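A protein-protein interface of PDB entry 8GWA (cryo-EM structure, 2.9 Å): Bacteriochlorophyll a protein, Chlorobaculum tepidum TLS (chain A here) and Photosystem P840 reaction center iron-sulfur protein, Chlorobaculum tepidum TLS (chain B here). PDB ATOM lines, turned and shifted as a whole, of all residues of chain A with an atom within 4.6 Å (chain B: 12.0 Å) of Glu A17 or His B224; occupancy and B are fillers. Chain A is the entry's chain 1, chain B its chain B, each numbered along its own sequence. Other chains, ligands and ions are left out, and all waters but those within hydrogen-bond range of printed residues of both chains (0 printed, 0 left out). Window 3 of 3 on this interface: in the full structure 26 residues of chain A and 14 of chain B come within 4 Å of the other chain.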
ATOM      1  N   ASP A  15     -28.756  -7.333  13.995  1.00  0.00           N
ATOM      2  CA  ASP A  15     -27.352  -7.708  14.085  1.00  0.00           C
ATOM      3  C   ASP A  15     -26.808  -7.967  12.689  1.00  0.00           C
ATOM      4  O   ASP A  15     -27.500  -8.537  11.842  1.00  0.00           O
ATOM      5  CB  ASP A  15     -27.146  -8.959  14.950  1.00  0.00           C
ATOM      6  CG  ASP A  15     -27.452  -8.720  16.412  1.00  0.00           C
ATOM      7  OD1 ASP A  15     -27.901  -7.612  16.766  1.00  0.00           O
ATOM      8  OD2 ASP A  15     -27.235  -9.652  17.213  1.00  0.00           O
ATOM      9  N   TYR A  16     -25.565  -7.551  12.457  1.00  0.00           N
ATOM     10  CA  TYR A  16     -24.897  -7.769  11.182  1.00  0.00           C
ATOM     11  C   TYR A  16     -23.495  -8.295  11.437  1.00  0.00           C
ATOM     12  O   TYR A  16     -22.807  -7.831  12.349  1.00  0.00           O
ATOM     13  CB  TYR A  16     -24.821  -6.479  10.357  1.00  0.00           C
ATOM     14  CG  TYR A  16     -26.077  -5.644  10.399  1.00  0.00           C
ATOM     15  CD1 TYR A  16     -27.244  -6.080   9.791  1.00  0.00           C
ATOM     16  CD2 TYR A  16     -26.096  -4.421  11.050  1.00  0.00           C
ATOM     17  CE1 TYR A  16     -28.393  -5.319   9.828  1.00  0.00           C
ATOM     18  CE2 TYR A  16     -27.239  -3.656  11.095  1.00  0.00           C
ATOM     19  CZ  TYR A  16     -28.383  -4.109  10.480  1.00  0.00           C
ATOM     20  OH  TYR A  16     -29.526  -3.348  10.520  1.00  0.00           O
ATOM     21  N   GLU A  17     -23.075  -9.268  10.631  1.00  0.00           N
ATOM     22  CA  GLU A  17     -21.738  -9.838  10.731  1.00  0.00           C
ATOM     23  C   GLU A  17     -21.122  -9.927   9.345  1.00  0.00           C
ATOM     24  O   GLU A  17     -21.792 -10.324   8.387  1.00  0.00           O
ATOM     25  CB  GLU A  17     -21.761 -11.222  11.383  1.00  0.00           C
ATOM     26  CG  GLU A  17     -20.418 -11.652  11.953  1.00  0.00           C
ATOM     27  CD  GLU A  17     -20.463 -13.030  12.581  1.00  0.00           C
ATOM     28  OE1 GLU A  17     -21.578 -13.555  12.784  1.00  0.00           O
ATOM     29  OE2 GLU A  17     -19.384 -13.588  12.872  1.00  0.00           O
ATOM     30  N   ILE A  18     -19.848  -9.556   9.244  1.00  0.00           N
ATOM     31  CA  ILE A  18     -19.075  -9.690   8.016  1.00  0.00           C
ATOM     32  C   ILE A  18     -17.802 -10.451   8.354  1.00  0.00           C
ATOM     33  O   ILE A  18     -17.001  -9.990   9.175  1.00  0.00           O
ATOM     34  CB  ILE A  18     -18.742  -8.327   7.388  1.00  0.00           C
ATOM     35  CG1 ILE A  18     -20.023  -7.556   7.066  1.00  0.00           C
ATOM     36  CG2 ILE A  18     -17.904  -8.509   6.137  1.00  0.00           C
ATOM     37  CD1 ILE A  18     -19.790  -6.098   6.750  1.00  0.00           C
ATOM     38  N   VAL A  19     -17.617 -11.609   7.728  1.00  0.00           N
ATOM     39  CA  VAL A  19     -16.442 -12.447   7.938  1.00  0.00           C
ATOM     40  C   VAL A  19     -15.687 -12.500   6.619  1.00  0.00           C
ATOM     41  O   VAL A  19     -16.086 -13.222   5.697  1.00  0.00           O
ATOM     42  CB  VAL A  19     -16.816 -13.856   8.418  1.00  0.00           C
ATOM     43  CG1 VAL A  19     -15.571 -14.720   8.550  1.00  0.00           C
ATOM     44  CG2 VAL A  19     -17.569 -13.784   9.735  1.00  0.00           C
ATOM     45  N   LYS A  29     -18.220 -13.944   4.339  1.00  0.00           N
ATOM     46  CA  LYS A  29     -19.504 -14.360   4.885  1.00  0.00           C
ATOM     47  C   LYS A  29     -20.284 -13.140   5.352  1.00  0.00           C
ATOM     48  O   LYS A  29     -19.759 -12.294   6.082  1.00  0.00           O
ATOM     49  CB  LYS A  29     -19.304 -15.331   6.046  1.00  0.00           C
ATOM     50  CG  LYS A  29     -18.368 -16.486   5.750  1.00  0.00           C
ATOM     51  CD  LYS A  29     -18.164 -17.343   6.988  1.00  0.00           C
ATOM     52  CE  LYS A  29     -17.445 -18.636   6.655  1.00  0.00           C
ATOM     53  NZ  LYS A  29     -18.331 -19.580   5.921  1.00  0.00           N
ATOM     54  N   VAL A  30     -21.540 -13.047   4.927  1.00  0.00           N
ATOM     55  CA  VAL A  30     -22.417 -11.943   5.297  1.00  0.00           C
ATOM     56  C   VAL A  30     -23.705 -12.528   5.849  1.00  0.00           C
ATOM     57  O   VAL A  30     -24.423 -13.240   5.137  1.00  0.00           O
ATOM     58  CB  VAL A  30     -22.713 -11.017   4.106  1.00  0.00           C
ATOM     59  CG1 VAL A  30     -23.820 -10.046   4.464  1.00  0.00           C
ATOM     60  CG2 VAL A  30     -21.461 -10.266   3.696  1.00  0.00           C
ATOM     61  N   LYS A  31     -24.003 -12.225   7.108  1.00  0.00           N
ATOM     62  CA  LYS A  31     -25.271 -12.609   7.702  1.00  0.00           C
ATOM     63  C   LYS A  31     -25.840 -11.426   8.469  1.00  0.00           C
ATOM     64  O   LYS A  31     -25.102 -10.640   9.069  1.00  0.00           O
ATOM     65  CB  LYS A  31     -25.137 -13.834   8.618  1.00  0.00           C
ATOM     66  CG  LYS A  31     -24.150 -13.681   9.756  1.00  0.00           C
ATOM     67  CD  LYS A  31     -23.894 -15.025  10.416  1.00  0.00           C
ATOM     68  CE  LYS A  31     -23.097 -15.941   9.503  1.00  0.00           C
ATOM     69  NZ  LYS A  31     -22.666 -17.185  10.197  1.00  0.00           N
ATOM     70  N   GLN A 312     -26.085  -3.730  15.880  1.00  0.00           N
ATOM     71  CA  GLN A 312     -24.712  -4.125  16.150  1.00  0.00           C
ATOM     72  C   GLN A 312     -24.122  -4.729  14.887  1.00  0.00           C
ATOM     73  O   GLN A 312     -24.699  -5.657  14.312  1.00  0.00           O
ATOM     74  CB  GLN A 312     -24.642  -5.129  17.303  1.00  0.00           C
ATOM     75  CG  GLN A 312     -23.270  -5.241  17.943  1.00  0.00           C
ATOM     76  CD  GLN A 312     -23.305  -5.987  19.259  1.00  0.00           C
ATOM     77  OE1 GLN A 312     -24.290  -6.642  19.587  1.00  0.00           O
ATOM     78  NE2 GLN A 312     -22.231  -5.880  20.029  1.00  0.00           N
ATOM     79  N   LYS A 314     -20.659  -6.471  13.060  1.00  0.00           N
ATOM     80  CA  LYS A 314     -19.470  -7.249  13.367  1.00  0.00           C
ATOM     81  C   LYS A 314     -18.676  -7.470  12.090  1.00  0.00           C
ATOM     82  O   LYS A 314     -19.208  -7.996  11.108  1.00  0.00           O
ATOM     83  CB  LYS A 314     -19.872  -8.577  14.000  1.00  0.00           C
ATOM     84  CG  LYS A 314     -20.538  -8.405  15.349  1.00  0.00           C
ATOM     85  CD  LYS A 314     -20.945  -9.734  15.922  1.00  0.00           C
ATOM     86  CE  LYS A 314     -22.145 -10.262  15.161  1.00  0.00           C
ATOM     87  NZ  LYS A 314     -23.343  -9.404  15.376  1.00  0.00           N
ATOM     88  N   VAL A 316     -15.146  -9.218  10.900  1.00  0.00           N
ATOM     89  CA  VAL A 316     -14.066 -10.113  11.294  1.00  0.00           C
ATOM     90  C   VAL A 316     -13.046 -10.101  10.162  1.00  0.00           C
ATOM     91  O   VAL A 316     -13.207 -10.794   9.154  1.00  0.00           O
ATOM     92  CB  VAL A 316     -14.577 -11.526  11.586  1.00  0.00           C
ATOM     93  CG1 VAL A 316     -13.455 -12.391  12.133  1.00  0.00           C
ATOM     94  CG2 VAL A 316     -15.742 -11.479  12.560  1.00  0.00           C
ATOM     95  N   ARG A 339     -16.323  -4.133  15.999  1.00  0.00           N
ATOM     96  CA  ARG A 339     -17.712  -4.160  16.428  1.00  0.00           C
ATOM     97  C   ARG A 339     -18.264  -2.745  16.453  1.00  0.00           C
ATOM     98  O   ARG A 339     -17.629  -1.837  16.997  1.00  0.00           O
ATOM     99  CB  ARG A 339     -17.826  -4.811  17.810  1.00  0.00           C
ATOM    100  CG  ARG A 339     -19.204  -5.306  18.179  1.00  0.00           C
ATOM    101  CD  ARG A 339     -19.133  -6.118  19.459  1.00  0.00           C
ATOM    102  NE  ARG A 339     -18.398  -7.364  19.286  1.00  0.00           N
ATOM    103  CZ  ARG A 339     -18.966  -8.537  19.042  1.00  0.00           C
ATOM    104  NH1 ARG A 339     -20.280  -8.661  18.944  1.00  0.00           N
ATOM    105  NH2 ARG A 339     -18.198  -9.614  18.901  1.00  0.00           N
ATOM    106  N   LEU B 220     -36.048 -16.817  14.877  1.00  0.00           N
ATOM    107  CA  LEU B 220     -35.172 -15.662  14.709  1.00  0.00           C
ATOM    108  C   LEU B 220     -34.171 -15.626  15.859  1.00  0.00           C
ATOM    109  O   LEU B 220     -34.529 -15.304  16.995  1.00  0.00           O
ATOM    110  CB  LEU B 220     -35.986 -14.373  14.651  1.00  0.00           C
ATOM    111  CG  LEU B 220     -35.183 -13.082  14.483  1.00  0.00           C
ATOM    112  CD1 LEU B 220     -34.362 -13.128  13.208  1.00  0.00           C
ATOM    113  CD2 LEU B 220     -36.099 -11.873  14.488  1.00  0.00           C
ATOM    114  N   ARG B 221     -32.917 -15.954  15.560  1.00  0.00           N
ATOM    115  CA  ARG B 221     -31.833 -15.925  16.532  1.00  0.00           C
ATOM    116  C   ARG B 221     -30.771 -14.949  16.055  1.00  0.00           C
ATOM    117  O   ARG B 221     -30.321 -15.029  14.908  1.00  0.00           O
ATOM    118  CB  ARG B 221     -31.237 -17.320  16.724  1.00  0.00           C
ATOM    119  CG  ARG B 221     -32.180 -18.300  17.398  1.00  0.00           C
ATOM    120  CD  ARG B 221     -31.949 -19.715  16.908  1.00  0.00           C
ATOM    121  NE  ARG B 221     -30.675 -20.259  17.356  1.00  0.00           N
ATOM    122  CZ  ARG B 221     -30.547 -21.210  18.270  1.00  0.00           C
ATOM    123  NH1 ARG B 221     -31.600 -21.723  18.884  1.00  0.00           N
ATOM    124  NH2 ARG B 221     -29.333 -21.659  18.573  1.00  0.00           N
ATOM    125  N   PHE B 222     -30.368 -14.036  16.933  1.00  0.00           N
ATOM    126  CA  PHE B 222     -29.446 -12.980  16.548  1.00  0.00           C
ATOM    127  C   PHE B 222     -28.011 -13.506  16.523  1.00  0.00           C
ATOM    128  O   PHE B 222     -27.734 -14.664  16.847  1.00  0.00           O
ATOM    129  CB  PHE B 222     -29.603 -11.780  17.477  1.00  0.00           C
ATOM    130  CG  PHE B 222     -30.807 -10.935  17.169  1.00  0.00           C
ATOM    131  CD1 PHE B 222     -32.083 -11.407  17.418  1.00  0.00           C
ATOM    132  CD2 PHE B 222     -30.661  -9.675  16.618  1.00  0.00           C
ATOM    133  CE1 PHE B 222     -33.190 -10.635  17.132  1.00  0.00           C
ATOM    134  CE2 PHE B 222     -31.766  -8.900  16.329  1.00  0.00           C
ATOM    135  CZ  PHE B 222     -33.031  -9.380  16.587  1.00  0.00           C
ATOM    136  N   LEU B 223     -27.081 -12.634  16.138  1.00  0.00           N
ATOM    137  CA  LEU B 223     -25.745 -13.061  15.725  1.00  0.00           C
ATOM    138  C   LEU B 223     -24.769 -13.164  16.894  1.00  0.00           C
ATOM    139  O   LEU B 223     -24.164 -14.219  17.109  1.00  0.00           O
ATOM    140  CB  LEU B 223     -25.207 -12.102  14.658  1.00  0.00           C
ATOM    141  CG  LEU B 223     -25.512 -12.434  13.197  1.00  0.00           C
ATOM    142  CD1 LEU B 223     -26.957 -12.833  12.998  1.00  0.00           C
ATOM    143  CD2 LEU B 223     -25.192 -11.236  12.338  1.00  0.00           C
ATOM    144  N   HIS B 224     -24.575 -12.070  17.633  1.00  0.00           N
ATOM    145  CA  HIS B 224     -23.743 -12.128  18.829  1.00  0.00           C
ATOM    146  C   HIS B 224     -24.304 -11.322  19.995  1.00  0.00           C
ATOM    147  O   HIS B 224     -23.541 -10.963  20.901  1.00  0.00           O
ATOM    148  CB  HIS B 224     -22.308 -11.683  18.523  1.00  0.00           C
ATOM    149  CG  HIS B 224     -21.474 -12.744  17.869  1.00  0.00           C
ATOM    150  ND1 HIS B 224     -21.535 -13.017  16.520  1.00  0.00           N
ATOM    151  CD2 HIS B 224     -20.562 -13.602  18.385  1.00  0.00           C
ATOM    152  CE1 HIS B 224     -20.694 -13.994  16.232  1.00  0.00           C
ATOM    153  NE2 HIS B 224     -20.093 -14.369  17.346  1.00  0.00           N
ATOM    154  N   ARG B 225     -25.600 -11.027  20.006  1.00  0.00           N
ATOM    155  CA  ARG B 225     -26.260 -10.520  21.197  1.00  0.00           C
ATOM    156  C   ARG B 225     -27.635 -11.159  21.288  1.00  0.00           C
ATOM    157  O   ARG B 225     -28.209 -11.587  20.283  1.00  0.00           O
ATOM    158  CB  ARG B 225     -26.388  -8.994  21.203  1.00  0.00           C
ATOM    159  CG  ARG B 225     -27.289  -8.444  20.117  1.00  0.00           C
ATOM    160  CD  ARG B 225     -27.327  -6.930  20.140  1.00  0.00           C
ATOM    161  NE  ARG B 225     -28.198  -6.402  19.098  1.00  0.00           N
ATOM    162  CZ  ARG B 225     -28.431  -5.113  18.898  1.00  0.00           C
ATOM    163  NH1 ARG B 225     -27.870  -4.184  19.655  1.00  0.00           N
ATOM    164  NH2 ARG B 225     -29.255  -4.746  17.922  1.00  0.00           N
ATOM    165  N   PHE B 226     -28.145 -11.224  22.518  1.00  0.00           N
ATOM    166  CA  PHE B 226     -29.383 -11.922  22.848  1.00  0.00           C
ATOM    167  C   PHE B 226     -29.171 -13.410  22.614  1.00  0.00           C
ATOM    168  O   PHE B 226     -29.048 -14.187  23.566  1.00  0.00           O
ATOM    169  CB  PHE B 226     -30.566 -11.405  22.022  1.00  0.00           C
ATOM    170  CG  PHE B 226     -30.695  -9.905  22.024  1.00  0.00           C
ATOM    171  CD1 PHE B 226     -31.040  -9.210  23.166  1.00  0.00           C
ATOM    172  CD2 PHE B 226     -30.537  -9.200  20.855  1.00  0.00           C
ATOM    173  CE1 PHE B 226     -31.146  -7.835  23.152  1.00  0.00           C
ATOM    174  CE2 PHE B 226     -30.662  -7.812  20.832  1.00  0.00           C
ATOM    175  CZ  PHE B 226     -30.967  -7.138  21.982  1.00  0.00           C
ATOM    176  N   HIS B 227     -29.137 -13.806  21.345  1.00  0.00           N
ATOM    177  CA  HIS B 227     -28.650 -15.108  20.926  1.00  0.00           C
ATOM    178  C   HIS B 227     -27.236 -14.977  20.372  1.00  0.00           C
ATOM    179  O   HIS B 227     -26.677 -13.885  20.268  1.00  0.00           O
ATOM    180  CB  HIS B 227     -29.561 -15.725  19.867  1.00  0.00           C
ATOM    181  CG  HIS B 227     -30.875 -16.194  20.393  1.00  0.00           C
ATOM    182  ND1 HIS B 227     -31.015 -17.369  21.100  1.00  0.00           N
ATOM    183  CD2 HIS B 227     -32.112 -15.653  20.309  1.00  0.00           C
ATOM    184  CE1 HIS B 227     -32.283 -17.534  21.426  1.00  0.00           C
ATOM    185  NE2 HIS B 227     -32.968 -16.506  20.959  1.00  0.00           N
ATOM    186  N   ARG B 228     -26.657 -16.117  19.996  1.00  0.00           N
ATOM    187  CA  ARG B 228     -25.413 -16.107  19.237  1.00  0.00           C
ATOM    188  C   ARG B 228     -25.438 -17.158  18.131  1.00  0.00           C
ATOM    189  O   ARG B 228     -24.383 -17.492  17.578  1.00  0.00           O
ATOM    190  CB  ARG B 228     -24.207 -16.297  20.169  1.00  0.00           C
ATOM    191  CG  ARG B 228     -23.846 -15.035  20.938  1.00  0.00           C
ATOM    192  CD  ARG B 228     -22.744 -15.253  21.957  1.00  0.00           C
ATOM    193  NE  ARG B 228     -22.401 -14.010  22.636  1.00  0.00           N
ATOM    194  CZ  ARG B 228     -23.150 -13.433  23.565  1.00  0.00           C
ATOM    195  NH1 ARG B 228     -24.296 -13.965  23.959  1.00  0.00           N
ATOM    196  NH2 ARG B 228     -22.742 -12.292  24.114  1.00  0.00           N
ATOM    197  N   GLU B 229     -26.625 -17.677  17.801  1.00  0.00           N
ATOM    198  CA  GLU B 229     -26.844 -18.635  16.712  1.00  0.00           C
ATOM    199  C   GLU B 229     -26.009 -19.879  16.991  1.00  0.00           C
ATOM    200  O   GLU B 229     -26.175 -20.472  18.072  1.00  0.00           O
ATOM    201  CB  GLU B 229     -26.583 -17.944  15.372  1.00  0.00           C
ATOM    202  CG  GLU B 229     -27.776 -17.171  14.836  1.00  0.00           C
ATOM    203  CD  GLU B 229     -28.709 -18.030  14.005  1.00  0.00           C
ATOM    204  OE1 GLU B 229     -28.602 -19.272  14.073  1.00  0.00           O
ATOM    205  OE2 GLU B 229     -29.553 -17.462  13.280  1.00  0.00           O
ATOM    206  N   ALA B 230     -25.127 -20.302  16.088  1.00  0.00           N
ATOM    207  CA  ALA B 230     -24.305 -21.498  16.266  1.00  0.00           C
ATOM    208  C   ALA B 230     -25.153 -22.727  16.588  1.00  0.00           C
ATOM    209  O   ALA B 230     -26.302 -22.829  16.156  1.00  0.00           O
ATOM    210  CB  ALA B 230     -23.262 -21.273  17.353  1.00  0.00           C
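N of Tyr A16 lies within hydrogen-bond range of O of Gln A312, at 2.8 Å. The backbone carbonyl oxygen of Tyr A16 sits at hydrogen-bond distance from the backbone NH of Lys A314 (2.6 Å). N of Glu A17 sits at hydrogen-bond distance from O of Lys A31, at 2.9 Å. The backbone carbonyl oxygen (O) of Lys A314 is in hydrogen-bond range of the backbone NH (N) of Ile A18 (2.5 Å). The backbone carbonyl oxygen (O) of Phe B222 lies close to the backbone NH (N) of Glu B229 (3.3 Å).
Printed residues of chain B within 4 Å of Tyr A16: Leu B223. Printed residues of chain B within 4 Å of Glu A17: Leu B223 and His B224. No residue of chain B comes within 4 Å of Ile A18. No residue of chain B comes within 4 Å of Val A19. Of chain B, only Leu B223 (3.3 Å) comes within 4 Å of Lys A31. Printed residues of chain B within 4 Å of Gln A312: Arg B225 (3.1 Å). Of the printed residues of chain B, Lys A314 touches Leu B223 and His B224. No residue of chain B comes within 4 Å of Val A316. Printed residues of chain A within 4 Å of Phe B222: Asp A15 (3.2 Å). Of chain A, only Asp A15 (3.6 Å), Glu A17 (3.6 Å), Lys A314 (3.1 Å) and Arg A339 (3.7 Å) come within 4 Å of His B224. The nearest residue of chain B that does not touch Glu A17 is Arg B228 (6.8 Å). The nearest printed residue of chain A that does not touch Phe B222 is Lys A314 (6.3 Å).
Among the printed residues, pairs that only touch across the chains: Asp A15 with Phe B222 (3.2 Å), Asp A15 with His B224 (3.6 Å), Tyr A16 with Leu B223 (3.5 Å), Glu A17 with Leu B223 (3.4 Å), Glu A17 with His B224 (3.6 Å), Lys A31 with Leu B223 (3.3 Å), Gln A312 with Arg B225 (3.1 Å), Lys A314 with Leu B223 (3.4 Å), Lys A314 with His B224 (3.1 Å) and Arg A339 with His B224 (3.7 Å).
The side-chain carboxylate of Asp A15 is in hydrogen-bond range of the backbone NH of Leu B223, 3.2 Å away. OD1 of Asp A15 lies within salt-bridge range of NE of Arg B225, 2.6 Å away.
Printed residues of chain B that touch a printed residue of chain A: Phe B222, Leu B223, His B224 and Arg B225. Hydrophobic or aromatic side chains of chain B within 4 Å of the printed part of chain A: Phe B222, Leu B223 and His B224. Along chain B the printed residues that touch a printed residue of chain A span positions 222 to 225. Of the 12 printed residues of chain A, 7 touch a printed residue of chain B.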
